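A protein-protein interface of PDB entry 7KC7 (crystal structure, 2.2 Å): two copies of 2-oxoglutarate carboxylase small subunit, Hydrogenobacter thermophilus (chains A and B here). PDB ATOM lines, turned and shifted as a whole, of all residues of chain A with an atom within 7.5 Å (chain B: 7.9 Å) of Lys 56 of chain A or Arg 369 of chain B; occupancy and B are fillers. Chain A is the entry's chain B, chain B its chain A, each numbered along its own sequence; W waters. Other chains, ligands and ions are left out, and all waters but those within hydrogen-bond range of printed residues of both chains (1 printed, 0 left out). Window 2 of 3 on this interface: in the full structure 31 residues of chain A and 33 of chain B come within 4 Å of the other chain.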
ATOM      1  N   CYS A  28     -26.297  -9.791  14.588  1.00  0.00           N
ATOM      2  CA  CYS A  28     -27.049  -9.745  15.860  1.00  0.00           C
ATOM      3  C   CYS A  28     -28.436 -10.373  15.741  1.00  0.00           C
ATOM      4  O   CYS A  28     -28.884 -11.055  16.671  1.00  0.00           O
ATOM      5  CB  CYS A  28     -27.167  -8.305  16.321  1.00  0.00           C
ATOM      6  SG  CYS A  28     -25.453  -7.640  16.694  1.00  0.00           S
ATOM      7  N   ILE A  31     -27.866 -14.127  15.846  1.00  0.00           N
ATOM      8  CA  ILE A  31     -27.459 -14.520  17.192  1.00  0.00           C
ATOM      9  C   ILE A  31     -28.673 -14.525  18.134  1.00  0.00           C
ATOM     10  O   ILE A  31     -28.847 -15.439  18.950  1.00  0.00           O
ATOM     11  CB  ILE A  31     -26.335 -13.585  17.703  1.00  0.00           C
ATOM     12  CG1 ILE A  31     -25.031 -13.894  16.972  1.00  0.00           C
ATOM     13  CG2 ILE A  31     -26.141 -13.746  19.212  1.00  0.00           C
ATOM     14  CD1 ILE A  31     -23.927 -12.861  17.239  1.00  0.00           C
ATOM     15  N   LYS A  35     -29.891 -17.624  20.233  1.00  0.00           N
ATOM     16  CA  LYS A  35     -30.008 -17.610  21.692  1.00  0.00           C
ATOM     17  C   LYS A  35     -31.404 -18.047  22.144  1.00  0.00           C
ATOM     18  O   LYS A  35     -31.546 -18.858  23.072  1.00  0.00           O
ATOM     19  CB  LYS A  35     -29.678 -16.217  22.239  1.00  0.00           C
ATOM     20  CG  LYS A  35     -28.202 -15.841  22.159  1.00  0.00           C
ATOM     21  CD  LYS A  35     -27.970 -14.392  22.577  1.00  0.00           C
ATOM     22  CE  LYS A  35     -28.270 -14.152  24.065  1.00  0.00           C
ATOM     23  NZ  LYS A  35     -27.332 -14.875  24.972  1.00  0.00           N
ATOM     24  N   ALA A  43     -19.130 -15.975  16.732  1.00  0.00           N
ATOM     25  CA  ALA A  43     -18.952 -14.822  15.873  1.00  0.00           C
ATOM     26  C   ALA A  43     -17.548 -14.835  15.275  1.00  0.00           C
ATOM     27  O   ALA A  43     -16.624 -15.416  15.846  1.00  0.00           O
ATOM     28  CB  ALA A  43     -19.180 -13.539  16.680  1.00  0.00           C
ATOM     29  N   SER A  50     -12.604  -4.968  16.973  1.00  0.00           N
ATOM     30  CA  SER A  50     -12.407  -5.835  18.104  1.00  0.00           C
ATOM     31  C   SER A  50     -13.568  -5.562  19.071  1.00  0.00           C
ATOM     32  O   SER A  50     -13.956  -6.441  19.815  1.00  0.00           O
ATOM     33  CB  SER A  50     -11.022  -5.546  18.679  1.00  0.00           C
ATOM     34  OG  SER A  50     -11.068  -5.735  20.041  1.00  0.00           O
ATOM     35  N   THR A  51     -14.247  -4.432  18.914  1.00  0.00           N
ATOM     36  CA  THR A  51     -15.305  -3.999  19.799  1.00  0.00           C
ATOM     37  C   THR A  51     -16.704  -4.215  19.259  1.00  0.00           C
ATOM     38  O   THR A  51     -17.629  -3.834  19.960  1.00  0.00           O
ATOM     39  CB  THR A  51     -15.205  -2.478  19.936  1.00  0.00           C
ATOM     40  OG1 THR A  51     -15.184  -1.985  18.556  1.00  0.00           O
ATOM     41  CG2 THR A  51     -13.993  -2.061  20.648  1.00  0.00           C
ATOM     42  N   ALA A  52     -16.895  -4.949  18.146  1.00  0.00           N
ATOM     43  CA  ALA A  52     -18.227  -5.022  17.552  1.00  0.00           C
ATOM     44  C   ALA A  52     -19.306  -5.595  18.470  1.00  0.00           C
ATOM     45  O   ALA A  52     -19.056  -6.501  19.267  1.00  0.00           O
ATOM     46  CB  ALA A  52     -18.201  -5.848  16.260  1.00  0.00           C
ATOM     47  N   ARG A  53     -20.553  -5.138  18.246  1.00  0.00           N
ATOM     48  CA  ARG A  53     -21.697  -5.586  19.048  1.00  0.00           C
ATOM     49  C   ARG A  53     -21.909  -7.086  18.871  1.00  0.00           C
ATOM     50  O   ARG A  53     -22.033  -7.826  19.851  1.00  0.00           O
ATOM     51  CB  ARG A  53     -22.963  -4.800  18.667  1.00  0.00           C
ATOM     52  CG  ARG A  53     -24.214  -5.182  19.487  1.00  0.00           C
ATOM     53  CD  ARG A  53     -23.984  -5.150  21.021  1.00  0.00           C
ATOM     54  NE  ARG A  53     -23.385  -3.904  21.486  1.00  0.00           N
ATOM     55  CZ  ARG A  53     -22.927  -3.707  22.721  1.00  0.00           C
ATOM     56  NH1 ARG A  53     -22.999  -4.673  23.635  1.00  0.00           N
ATOM     57  NH2 ARG A  53     -22.417  -2.535  23.043  1.00  0.00           N
ATOM     58  N   HIS A  54     -21.840  -7.574  17.630  1.00  0.00           N
ATOM     59  CA  HIS A  54     -22.052  -8.997  17.388  1.00  0.00           C
ATOM     60  C   HIS A  54     -20.962  -9.811  18.074  1.00  0.00           C
ATOM     61  O   HIS A  54     -21.206 -10.952  18.492  1.00  0.00           O
ATOM     62  CB  HIS A  54     -22.147  -9.296  15.871  1.00  0.00           C
ATOM     63  CG  HIS A  54     -20.843  -9.258  15.142  1.00  0.00           C
ATOM     64  ND1 HIS A  54     -20.198  -8.082  14.835  1.00  0.00           N
ATOM     65  CD2 HIS A  54     -20.071 -10.257  14.636  1.00  0.00           C
ATOM     66  CE1 HIS A  54     -19.056  -8.357  14.225  1.00  0.00           C
ATOM     67  NE2 HIS A  54     -18.955  -9.668  14.091  1.00  0.00           N
ATOM     68  N   VAL A  55     -19.784  -9.226  18.287  1.00  0.00           N
ATOM     69  CA  VAL A  55     -18.764  -9.981  19.009  1.00  0.00           C
ATOM     70  C   VAL A  55     -19.163 -10.136  20.479  1.00  0.00           C
ATOM     71  O   VAL A  55     -19.049 -11.230  21.065  1.00  0.00           O
ATOM     72  CB  VAL A  55     -17.394  -9.302  18.834  1.00  0.00           C
ATOM     73  CG1 VAL A  55     -16.347  -9.893  19.809  1.00  0.00           C
ATOM     74  CG2 VAL A  55     -16.933  -9.398  17.349  1.00  0.00           C
ATOM     75  N   LYS A  56     -19.710  -9.074  21.080  1.00  0.00           N
ATOM     76  CA  LYS A  56     -20.113  -9.138  22.484  1.00  0.00           C
ATOM     77  C   LYS A  56     -21.361  -9.990  22.700  1.00  0.00           C
ATOM     78  O   LYS A  56     -21.570 -10.506  23.816  1.00  0.00           O
ATOM     79  CB  LYS A  56     -20.357  -7.707  22.975  1.00  0.00           C
ATOM     80  CG  LYS A  56     -19.136  -6.891  22.791  1.00  0.00           C
ATOM     81  CD  LYS A  56     -19.362  -5.468  23.201  1.00  0.00           C
ATOM     82  CE  LYS A  56     -18.022  -4.796  23.404  1.00  0.00           C
ATOM     83  NZ  LYS A  56     -18.237  -3.565  24.183  1.00  0.00           N
ATOM     84  N   MET A  57     -22.243 -10.073  21.695  1.00  0.00           N
ATOM     85  CA  MET A  57     -23.461 -10.852  21.874  1.00  0.00           C
ATOM     86  C   MET A  57     -23.160 -12.357  21.763  1.00  0.00           C
ATOM     87  O   MET A  57     -23.817 -13.154  22.425  1.00  0.00           O
ATOM     88  CB  MET A  57     -24.508 -10.439  20.820  1.00  0.00           C
ATOM     89  CG  MET A  57     -25.016  -8.998  20.938  1.00  0.00           C
ATOM     90  SD  MET A  57     -26.559  -8.635  20.089  1.00  0.00           S
ATOM     91  CE  MET A  57     -27.063 -10.259  19.625  1.00  0.00           C
ATOM     92  N   ALA A  58     -22.148 -12.778  21.005  1.00  0.00           N
ATOM     93  CA  ALA A  58     -21.973 -14.210  20.758  1.00  0.00           C
ATOM     94  C   ALA A  58     -21.363 -14.870  21.994  1.00  0.00           C
ATOM     95  O   ALA A  58     -20.754 -14.216  22.833  1.00  0.00           O
ATOM     96  CB  ALA A  58     -21.083 -14.416  19.520  1.00  0.00           C
ATOM     97  N   ASP A  59     -21.595 -16.176  22.128  1.00  0.00           N
ATOM     98  CA  ASP A  59     -20.944 -16.941  23.196  1.00  0.00           C
ATOM     99  C   ASP A  59     -19.438 -17.081  22.967  1.00  0.00           C
ATOM    100  O   ASP A  59     -18.683 -17.198  23.928  1.00  0.00           O
ATOM    101  CB  ASP A  59     -21.586 -18.323  23.325  1.00  0.00           C
ATOM    102  CG  ASP A  59     -23.127 -18.252  23.599  1.00  0.00           C
ATOM    103  OD1 ASP A  59     -23.572 -17.551  24.538  1.00  0.00           O
ATOM    104  OD2 ASP A  59     -23.894 -18.909  22.875  1.00  0.00           O
ATOM    105  N   GLU A  60     -18.970 -17.077  21.723  1.00  0.00           N
ATOM    106  CA  GLU A  60     -17.532 -17.114  21.496  1.00  0.00           C
ATOM    107  C   GLU A  60     -17.227 -16.422  20.171  1.00  0.00           C
ATOM    108  O   GLU A  60     -18.033 -16.452  19.241  1.00  0.00           O
ATOM    109  CB  GLU A  60     -17.037 -18.564  21.567  1.00  0.00           C
ATOM    110  CG  GLU A  60     -17.575 -19.589  20.570  1.00  0.00           C
ATOM    111  CD  GLU A  60     -16.932 -20.968  20.806  1.00  0.00           C
ATOM    112  OE1 GLU A  60     -17.599 -21.839  21.391  1.00  0.00           O
ATOM    113  OE2 GLU A  60     -15.725 -21.173  20.475  1.00  0.00           O
ATOM    114  N   ALA A  61     -16.066 -15.777  20.097  1.00  0.00           N
ATOM    115  CA  ALA A  61     -15.749 -14.932  18.958  1.00  0.00           C
ATOM    116  C   ALA A  61     -14.278 -15.068  18.564  1.00  0.00           C
ATOM    117  O   ALA A  61     -13.398 -15.103  19.418  1.00  0.00           O
ATOM    118  CB  ALA A  61     -16.069 -13.478  19.306  1.00  0.00           C
ATOM    119  N   SER A 385     -24.068   1.748  19.156  1.00  0.00           N
ATOM    120  CA  SER A 385     -24.027   2.426  20.446  1.00  0.00           C
ATOM    121  C   SER A 385     -23.199   3.694  20.274  1.00  0.00           C
ATOM    122  O   SER A 385     -22.500   3.845  19.267  1.00  0.00           O
ATOM    123  CB  SER A 385     -23.349   1.590  21.534  1.00  0.00           C
ATOM    124  OG  SER A 385     -24.066   0.433  21.875  1.00  0.00           O
ATOM    125  N   LYS A 386     -23.120   4.519  21.331  1.00  0.00           N
ATOM    126  CA  LYS A 386     -22.174   5.632  21.296  1.00  0.00           C
ATOM    127  C   LYS A 386     -20.788   5.066  21.037  1.00  0.00           C
ATOM    128  O   LYS A 386     -20.402   4.064  21.637  1.00  0.00           O
ATOM    129  CB  LYS A 386     -22.154   6.410  22.607  1.00  0.00           C
ATOM    130  CG  LYS A 386     -21.242   7.662  22.546  1.00  0.00           C
ATOM    131  CD  LYS A 386     -20.243   7.672  23.683  1.00  0.00           C
ATOM    132  CE  LYS A 386     -19.115   8.645  23.408  1.00  0.00           C
ATOM    133  NZ  LYS A 386     -19.739  10.008  23.351  1.00  0.00           N
ATOM    134  N   THR B 366     -24.157   7.705  36.664  1.00  0.00           N
ATOM    135  CA  THR B 366     -24.397   8.040  35.275  1.00  0.00           C
ATOM    136  C   THR B 366     -24.158   6.831  34.379  1.00  0.00           C
ATOM    137  O   THR B 366     -23.274   6.002  34.629  1.00  0.00           O
ATOM    138  CB  THR B 366     -23.498   9.206  34.843  1.00  0.00           C
ATOM    139  OG1 THR B 366     -23.997  10.412  35.425  1.00  0.00           O
ATOM    140  CG2 THR B 366     -23.463   9.386  33.310  1.00  0.00           C
ATOM    141  N   ILE B 367     -24.997   6.725  33.351  1.00  0.00           N
ATOM    142  CA  ILE B 367     -24.886   5.636  32.399  1.00  0.00           C
ATOM    143  C   ILE B 367     -23.692   5.894  31.498  1.00  0.00           C
ATOM    144  O   ILE B 367     -23.541   6.984  30.925  1.00  0.00           O
ATOM    145  CB  ILE B 367     -26.181   5.504  31.593  1.00  0.00           C
ATOM    146  CG1 ILE B 367     -27.310   5.052  32.546  1.00  0.00           C
ATOM    147  CG2 ILE B 367     -26.015   4.501  30.468  1.00  0.00           C
ATOM    148  CD1 ILE B 367     -28.615   4.863  31.872  1.00  0.00           C
ATOM    149  N   GLU B 368     -22.865   4.879  31.341  1.00  0.00           N
ATOM    150  CA  GLU B 368     -21.706   4.934  30.462  1.00  0.00           C
ATOM    151  C   GLU B 368     -22.011   4.140  29.194  1.00  0.00           C
ATOM    152  O   GLU B 368     -22.415   4.724  28.173  1.00  0.00           O
ATOM    153  CB  GLU B 368     -20.463   4.394  31.183  1.00  0.00           C
ATOM    154  CG  GLU B 368     -19.867   5.328  32.248  1.00  0.00           C
ATOM    155  CD  GLU B 368     -18.870   4.626  33.190  1.00  0.00           C
ATOM    156  OE1 GLU B 368     -18.806   5.011  34.380  1.00  0.00           O
ATOM    157  OE2 GLU B 368     -18.161   3.685  32.739  1.00  0.00           O
ATOM    158  N   ARG B 369     -21.838   2.815  29.245  1.00  0.00           N
ATOM    159  CA  ARG B 369     -22.233   1.961  28.127  1.00  0.00           C
ATOM    160  C   ARG B 369     -23.739   1.693  28.151  1.00  0.00           C
ATOM    161  O   ARG B 369     -24.360   1.524  29.216  1.00  0.00           O
ATOM    162  CB  ARG B 369     -21.439   0.665  28.150  1.00  0.00           C
ATOM    163  CG  ARG B 369     -20.002   0.895  27.667  1.00  0.00           C
ATOM    164  CD  ARG B 369     -19.079  -0.281  27.955  1.00  0.00           C
ATOM    165  NE  ARG B 369     -17.890  -0.199  27.108  1.00  0.00           N
ATOM    166  CZ  ARG B 369     -17.876  -0.598  25.840  1.00  0.00           C
ATOM    167  NH1 ARG B 369     -19.003  -1.076  25.293  1.00  0.00           N
ATOM    168  NH2 ARG B 369     -16.759  -0.491  25.115  1.00  0.00           N
ATOM    169  N   TYR B 370     -24.330   1.779  26.963  1.00  0.00           N
ATOM    170  CA  TYR B 370     -25.766   1.669  26.801  1.00  0.00           C
ATOM    171  C   TYR B 370     -26.047   1.122  25.411  1.00  0.00           C
ATOM    172  O   TYR B 370     -25.943   1.862  24.411  1.00  0.00           O
ATOM    173  CB  TYR B 370     -26.441   3.005  26.991  1.00  0.00           C
ATOM    174  CG  TYR B 370     -27.928   2.889  27.214  1.00  0.00           C
ATOM    175  CD1 TYR B 370     -28.425   2.362  28.402  1.00  0.00           C
ATOM    176  CD2 TYR B 370     -28.830   3.314  26.244  1.00  0.00           C
ATOM    177  CE1 TYR B 370     -29.769   2.273  28.633  1.00  0.00           C
ATOM    178  CE2 TYR B 370     -30.184   3.237  26.450  1.00  0.00           C
ATOM    179  CZ  TYR B 370     -30.662   2.705  27.658  1.00  0.00           C
ATOM    180  OH  TYR B 370     -31.989   2.589  27.917  1.00  0.00           O
ATOM    181  N   TYR B 371     -26.388  -0.163  25.363  1.00  0.00           N
ATOM    182  CA  TYR B 371     -26.910  -0.786  24.158  1.00  0.00           C
ATOM    183  C   TYR B 371     -28.261  -1.416  24.466  1.00  0.00           C
ATOM    184  O   TYR B 371     -28.384  -2.304  25.327  1.00  0.00           O
ATOM    185  CB  TYR B 371     -25.953  -1.837  23.592  1.00  0.00           C
ATOM    186  CG  TYR B 371     -26.549  -2.622  22.466  1.00  0.00           C
ATOM    187  CD1 TYR B 371     -26.627  -2.103  21.167  1.00  0.00           C
ATOM    188  CD2 TYR B 371     -27.121  -3.860  22.708  1.00  0.00           C
ATOM    189  CE1 TYR B 371     -27.213  -2.846  20.121  1.00  0.00           C
ATOM    190  CE2 TYR B 371     -27.720  -4.591  21.703  1.00  0.00           C
ATOM    191  CZ  TYR B 371     -27.757  -4.095  20.406  1.00  0.00           C
ATOM    192  OH  TYR B 371     -28.322  -4.877  19.444  1.00  0.00           O
ATOM    193  N   VAL B 372     -29.243  -0.994  23.692  1.00  0.00           N
ATOM    194  CA  VAL B 372     -30.638  -1.396  23.825  1.00  0.00           C
ATOM    195  C   VAL B 372     -30.896  -2.539  22.852  1.00  0.00           C
ATOM    196  O   VAL B 372     -30.608  -2.399  21.662  1.00  0.00           O
ATOM    197  CB  VAL B 372     -31.586  -0.209  23.566  1.00  0.00           C
ATOM    198  CG1 VAL B 372     -31.279   0.488  22.263  1.00  0.00           C
ATOM    199  CG2 VAL B 372     -33.040  -0.640  23.469  1.00  0.00           C
ATOM    200  N   SER B 385     -29.825   7.335  27.526  1.00  0.00           N
ATOM    201  CA  SER B 385     -28.713   7.290  26.611  1.00  0.00           C
ATOM    202  C   SER B 385     -27.436   7.291  27.451  1.00  0.00           C
ATOM    203  O   SER B 385     -27.487   7.447  28.676  1.00  0.00           O
ATOM    204  CB  SER B 385     -28.747   8.505  25.704  1.00  0.00           C
ATOM    205  OG  SER B 385     -29.922   8.510  24.928  1.00  0.00           O
ATOM    206  N   LYS B 386     -26.275   7.204  26.794  1.00  0.00           N
ATOM    207  CA  LYS B 386     -25.027   7.411  27.529  1.00  0.00           C
ATOM    208  C   LYS B 386     -25.103   8.781  28.181  1.00  0.00           C
ATOM    209  O   LYS B 386     -25.567   9.736  27.553  1.00  0.00           O
ATOM    210  CB  LYS B 386     -23.814   7.338  26.611  1.00  0.00           C
ATOM    211  CG  LYS B 386     -22.496   7.658  27.319  1.00  0.00           C
ATOM    212  N   GLY B 387     -24.751   8.856  29.469  1.00  0.00           N
ATOM    213  CA  GLY B 387     -24.766  10.110  30.203  1.00  0.00           C
ATOM    214  C   GLY B 387     -26.043  10.458  30.942  1.00  0.00           C
ATOM    215  O   GLY B 387     -26.063  11.479  31.640  1.00  0.00           O
ATOM    216  N   GLU B 420     -29.850 -10.717  28.232  1.00  0.00           N
ATOM    217  CA  GLU B 420     -28.429 -11.080  28.175  1.00  0.00           C
ATOM    218  C   GLU B 420     -27.637 -10.178  27.230  1.00  0.00           C
ATOM    219  O   GLU B 420     -26.408 -10.163  27.297  1.00  0.00           O
ATOM    220  CB  GLU B 420     -28.238 -12.538  27.735  1.00  0.00           C
ATOM    221  CG  GLU B 420     -28.475 -13.481  28.871  1.00  0.00           C
ATOM    222  CD  GLU B 420     -28.603 -14.901  28.396  1.00  0.00           C
ATOM    223  OE1 GLU B 420     -28.775 -15.092  27.161  1.00  0.00           O
ATOM    224  OE2 GLU B 420     -28.512 -15.812  29.259  1.00  0.00           O
ATOM    225  N   THR B 421     -28.316  -9.405  26.379  1.00  0.00           N
ATOM    226  CA  THR B 421     -27.672  -8.485  25.454  1.00  0.00           C
ATOM    227  C   THR B 421     -27.854  -7.020  25.792  1.00  0.00           C
ATOM    228  O   THR B 421     -27.332  -6.176  25.063  1.00  0.00           O
ATOM    229  CB  THR B 421     -28.247  -8.732  24.053  1.00  0.00           C
ATOM    230  OG1 THR B 421     -29.687  -8.489  24.066  1.00  0.00           O
ATOM    231  CG2 THR B 421     -27.954 -10.168  23.612  1.00  0.00           C
ATOM    232  N   TYR B 422     -28.586  -6.689  26.858  1.00  0.00           N
ATOM    233  CA  TYR B 422     -28.864  -5.302  27.211  1.00  0.00           C
ATOM    234  C   TYR B 422     -27.676  -4.815  28.026  1.00  0.00           C
ATOM    235  O   TYR B 422     -27.589  -5.128  29.206  1.00  0.00           O
ATOM    236  CB  TYR B 422     -30.163  -5.203  28.035  1.00  0.00           C
ATOM    237  CG  TYR B 422     -30.836  -3.854  28.016  1.00  0.00           C
ATOM    238  CD1 TYR B 422     -30.097  -2.670  27.943  1.00  0.00           C
ATOM    239  CD2 TYR B 422     -32.223  -3.760  28.043  1.00  0.00           C
ATOM    240  CE1 TYR B 422     -30.729  -1.439  27.888  1.00  0.00           C
ATOM    241  CE2 TYR B 422     -32.856  -2.554  28.000  1.00  0.00           C
ATOM    242  CZ  TYR B 422     -32.123  -1.393  27.923  1.00  0.00           C
ATOM    243  OH  TYR B 422     -32.816  -0.205  27.875  1.00  0.00           O
ATOM    244  N   GLU B 423     -26.804  -3.996  27.447  1.00  0.00           N
ATOM    245  CA  GLU B 423     -25.565  -3.591  28.108  1.00  0.00           C
ATOM    246  C   GLU B 423     -25.716  -2.229  28.752  1.00  0.00           C
ATOM    247  O   GLU B 423     -25.974  -1.233  28.058  1.00  0.00           O
ATOM    248  CB  GLU B 423     -24.403  -3.571  27.109  1.00  0.00           C
ATOM    249  CG  GLU B 423     -23.025  -3.185  27.758  1.00  0.00           C
ATOM    250  CD  GLU B 423     -21.811  -3.158  26.779  1.00  0.00           C
ATOM    251  OE1 GLU B 423     -20.776  -3.782  27.089  1.00  0.00           O
ATOM    252  OE2 GLU B 423     -21.889  -2.511  25.721  1.00  0.00           O
ATOM    253  N   ILE B 424     -25.557  -2.187  30.080  1.00  0.00           N
ATOM    254  CA  ILE B 424     -25.588  -0.918  30.793  1.00  0.00           C
ATOM    255  C   ILE B 424     -24.449  -0.906  31.803  1.00  0.00           C
ATOM    256  O   ILE B 424     -24.360  -1.816  32.630  1.00  0.00           O
ATOM    257  CB  ILE B 424     -26.931  -0.701  31.516  1.00  0.00           C
ATOM    258  CG1 ILE B 424     -28.112  -0.860  30.537  1.00  0.00           C
ATOM    259  CG2 ILE B 424     -26.869   0.579  32.308  1.00  0.00           C
ATOM    260  CD1 ILE B 424     -29.408  -0.782  31.282  1.00  0.00           C
ATOM    261  N   SER B 425     -23.604   0.129  31.772  1.00  0.00           N
ATOM    262  CA  SER B 425     -22.543   0.288  32.769  1.00  0.00           C
ATOM    263  C   SER B 425     -22.611   1.691  33.361  1.00  0.00           C
ATOM    264  O   SER B 425     -23.249   2.589  32.801  1.00  0.00           O
ATOM    265  CB  SER B 425     -21.164   0.028  32.144  1.00  0.00           C
ATOM    266  OG  SER B 425     -20.740   1.154  31.389  1.00  0.00           O
ATOM    267  N   GLY B 426     -21.911   1.867  34.488  1.00  0.00           N
ATOM    268  CA  GLY B 426     -21.874   3.110  35.234  1.00  0.00           C
ATOM    269  C   GLY B 426     -22.765   3.126  36.472  1.00  0.00           C
ATOM    270  O   GLY B 426     -22.586   3.977  37.354  1.00  0.00           O
ATOM    271  N   VAL B 427     -23.705   2.200  36.558  1.00  0.00           N
ATOM    272  CA  VAL B 427     -24.553   2.049  37.718  1.00  0.00           C
ATOM    273  C   VAL B 427     -24.850   0.569  37.775  1.00  0.00           C
ATOM    274  O   VAL B 427     -24.805  -0.138  36.761  1.00  0.00           O
ATOM    275  CB  VAL B 427     -25.851   2.888  37.641  1.00  0.00           C
ATOM    276  CG1 VAL B 427     -25.524   4.370  37.621  1.00  0.00           C
ATOM    277  CG2 VAL B 427     -26.689   2.483  36.412  1.00  0.00           C
HETATM  278  O   HOH W   1     -24.819   4.367  23.505  1.00  0.00           O
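NH2 of Arg 53 of chain A is in salt-bridge range of OE2 of Glu 423 of chain B, at 2.7 Å. The side-chain amino group (NZ) of Lys 56 of chain A sits close to the guanidinium group (NH1) of Arg 369 of chain B, 2.8 Å away. The side-chain carboxylate (OE1) of Glu 420 of chain B is in salt-bridge range of the side-chain amino group (NZ) of Lys 35 of chain A, 2.6 Å away. The backbone carbonyl oxygen (O) of Tyr 370 of chain B lies within hydrogen-bond range of the side-chain hydroxyl (OG) of Ser 385 of chain A (3.5 Å). The side-chain amino group (NZ) of Lys 56 of chain A is in salt-bridge range of the side-chain carboxylate (OE1) of Glu 423 of chain B (3.9 Å).
The backbone NH (N) of Arg 369 of chain B sits at hydrogen-bond distance from the side-chain hydroxyl (OG) of Ser 425 of chain B. The backbone carbonyl oxygen of Glu 423 of chain B lies within hydrogen-bond range of the backbone NH of Tyr 371 of chain B (2.9 Å). The guanidinium group (NH1) of Arg 369 of chain B is in salt-bridge range of the side-chain carboxylate (OE2) of Glu 423 of chain B (3.3 Å). The side-chain hydroxyl of Tyr 422 of chain B lies within hydrogen-bond range of the side-chain hydroxyl of Tyr 370 of chain B.
Tyr 371 of chain B touches Arg 53 of chain A. Tyr 371 of chain B touches Ser 385 of chain A (CB to OG, 3.4 Å).
Of the printed residues of chain B, Lys 35 of chain A touches Glu 420. Of the printed residues of chain B, Arg 53 of chain A touches Tyr 371 and Glu 423. His 54 of chain A touches none of the printed residues of chain B. Lys 56 of chain A touches just these residues of chain B: Arg 369 (2.8 Å) and Glu 423 (3.9 Å). Arg 369 of chain B touches just one residue of chain A: Lys 56 (2.8 Å). Of the printed residues of chain A, Tyr 371 of chain B touches Arg 53 and Ser 385. Printed residues of chain A within 4 Å of Glu 423 of chain B: Arg 53 and Lys 56. The nearest residue of chain B that does not touch Lys 56 of chain A is Glu 420 of chain B (6.0 Å).
Of the 18 printed residues of chain B, 5 touch a printed residue of chain A. Hydrophobic or aromatic side chains of chain B that line the printed part of chain A: Tyr 371. Printed residues of chain A that touch a printed residue of chain B: Lys 35, Arg 53, Lys 56 and Ser 385. Among the printed residues, 7 pairs touch across the chains.
2 positions are printed for both chains. Of the 7 pairs that touch across the chains among the printed residues, none has its exchanged pair printed and touching as well.
Water W1 bridges the backbone NH (N) of Lys 386 of chain A (2.8 Å) and the backbone carbonyl oxygen (O) of Tyr 370 of chain B (2.9 Å).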
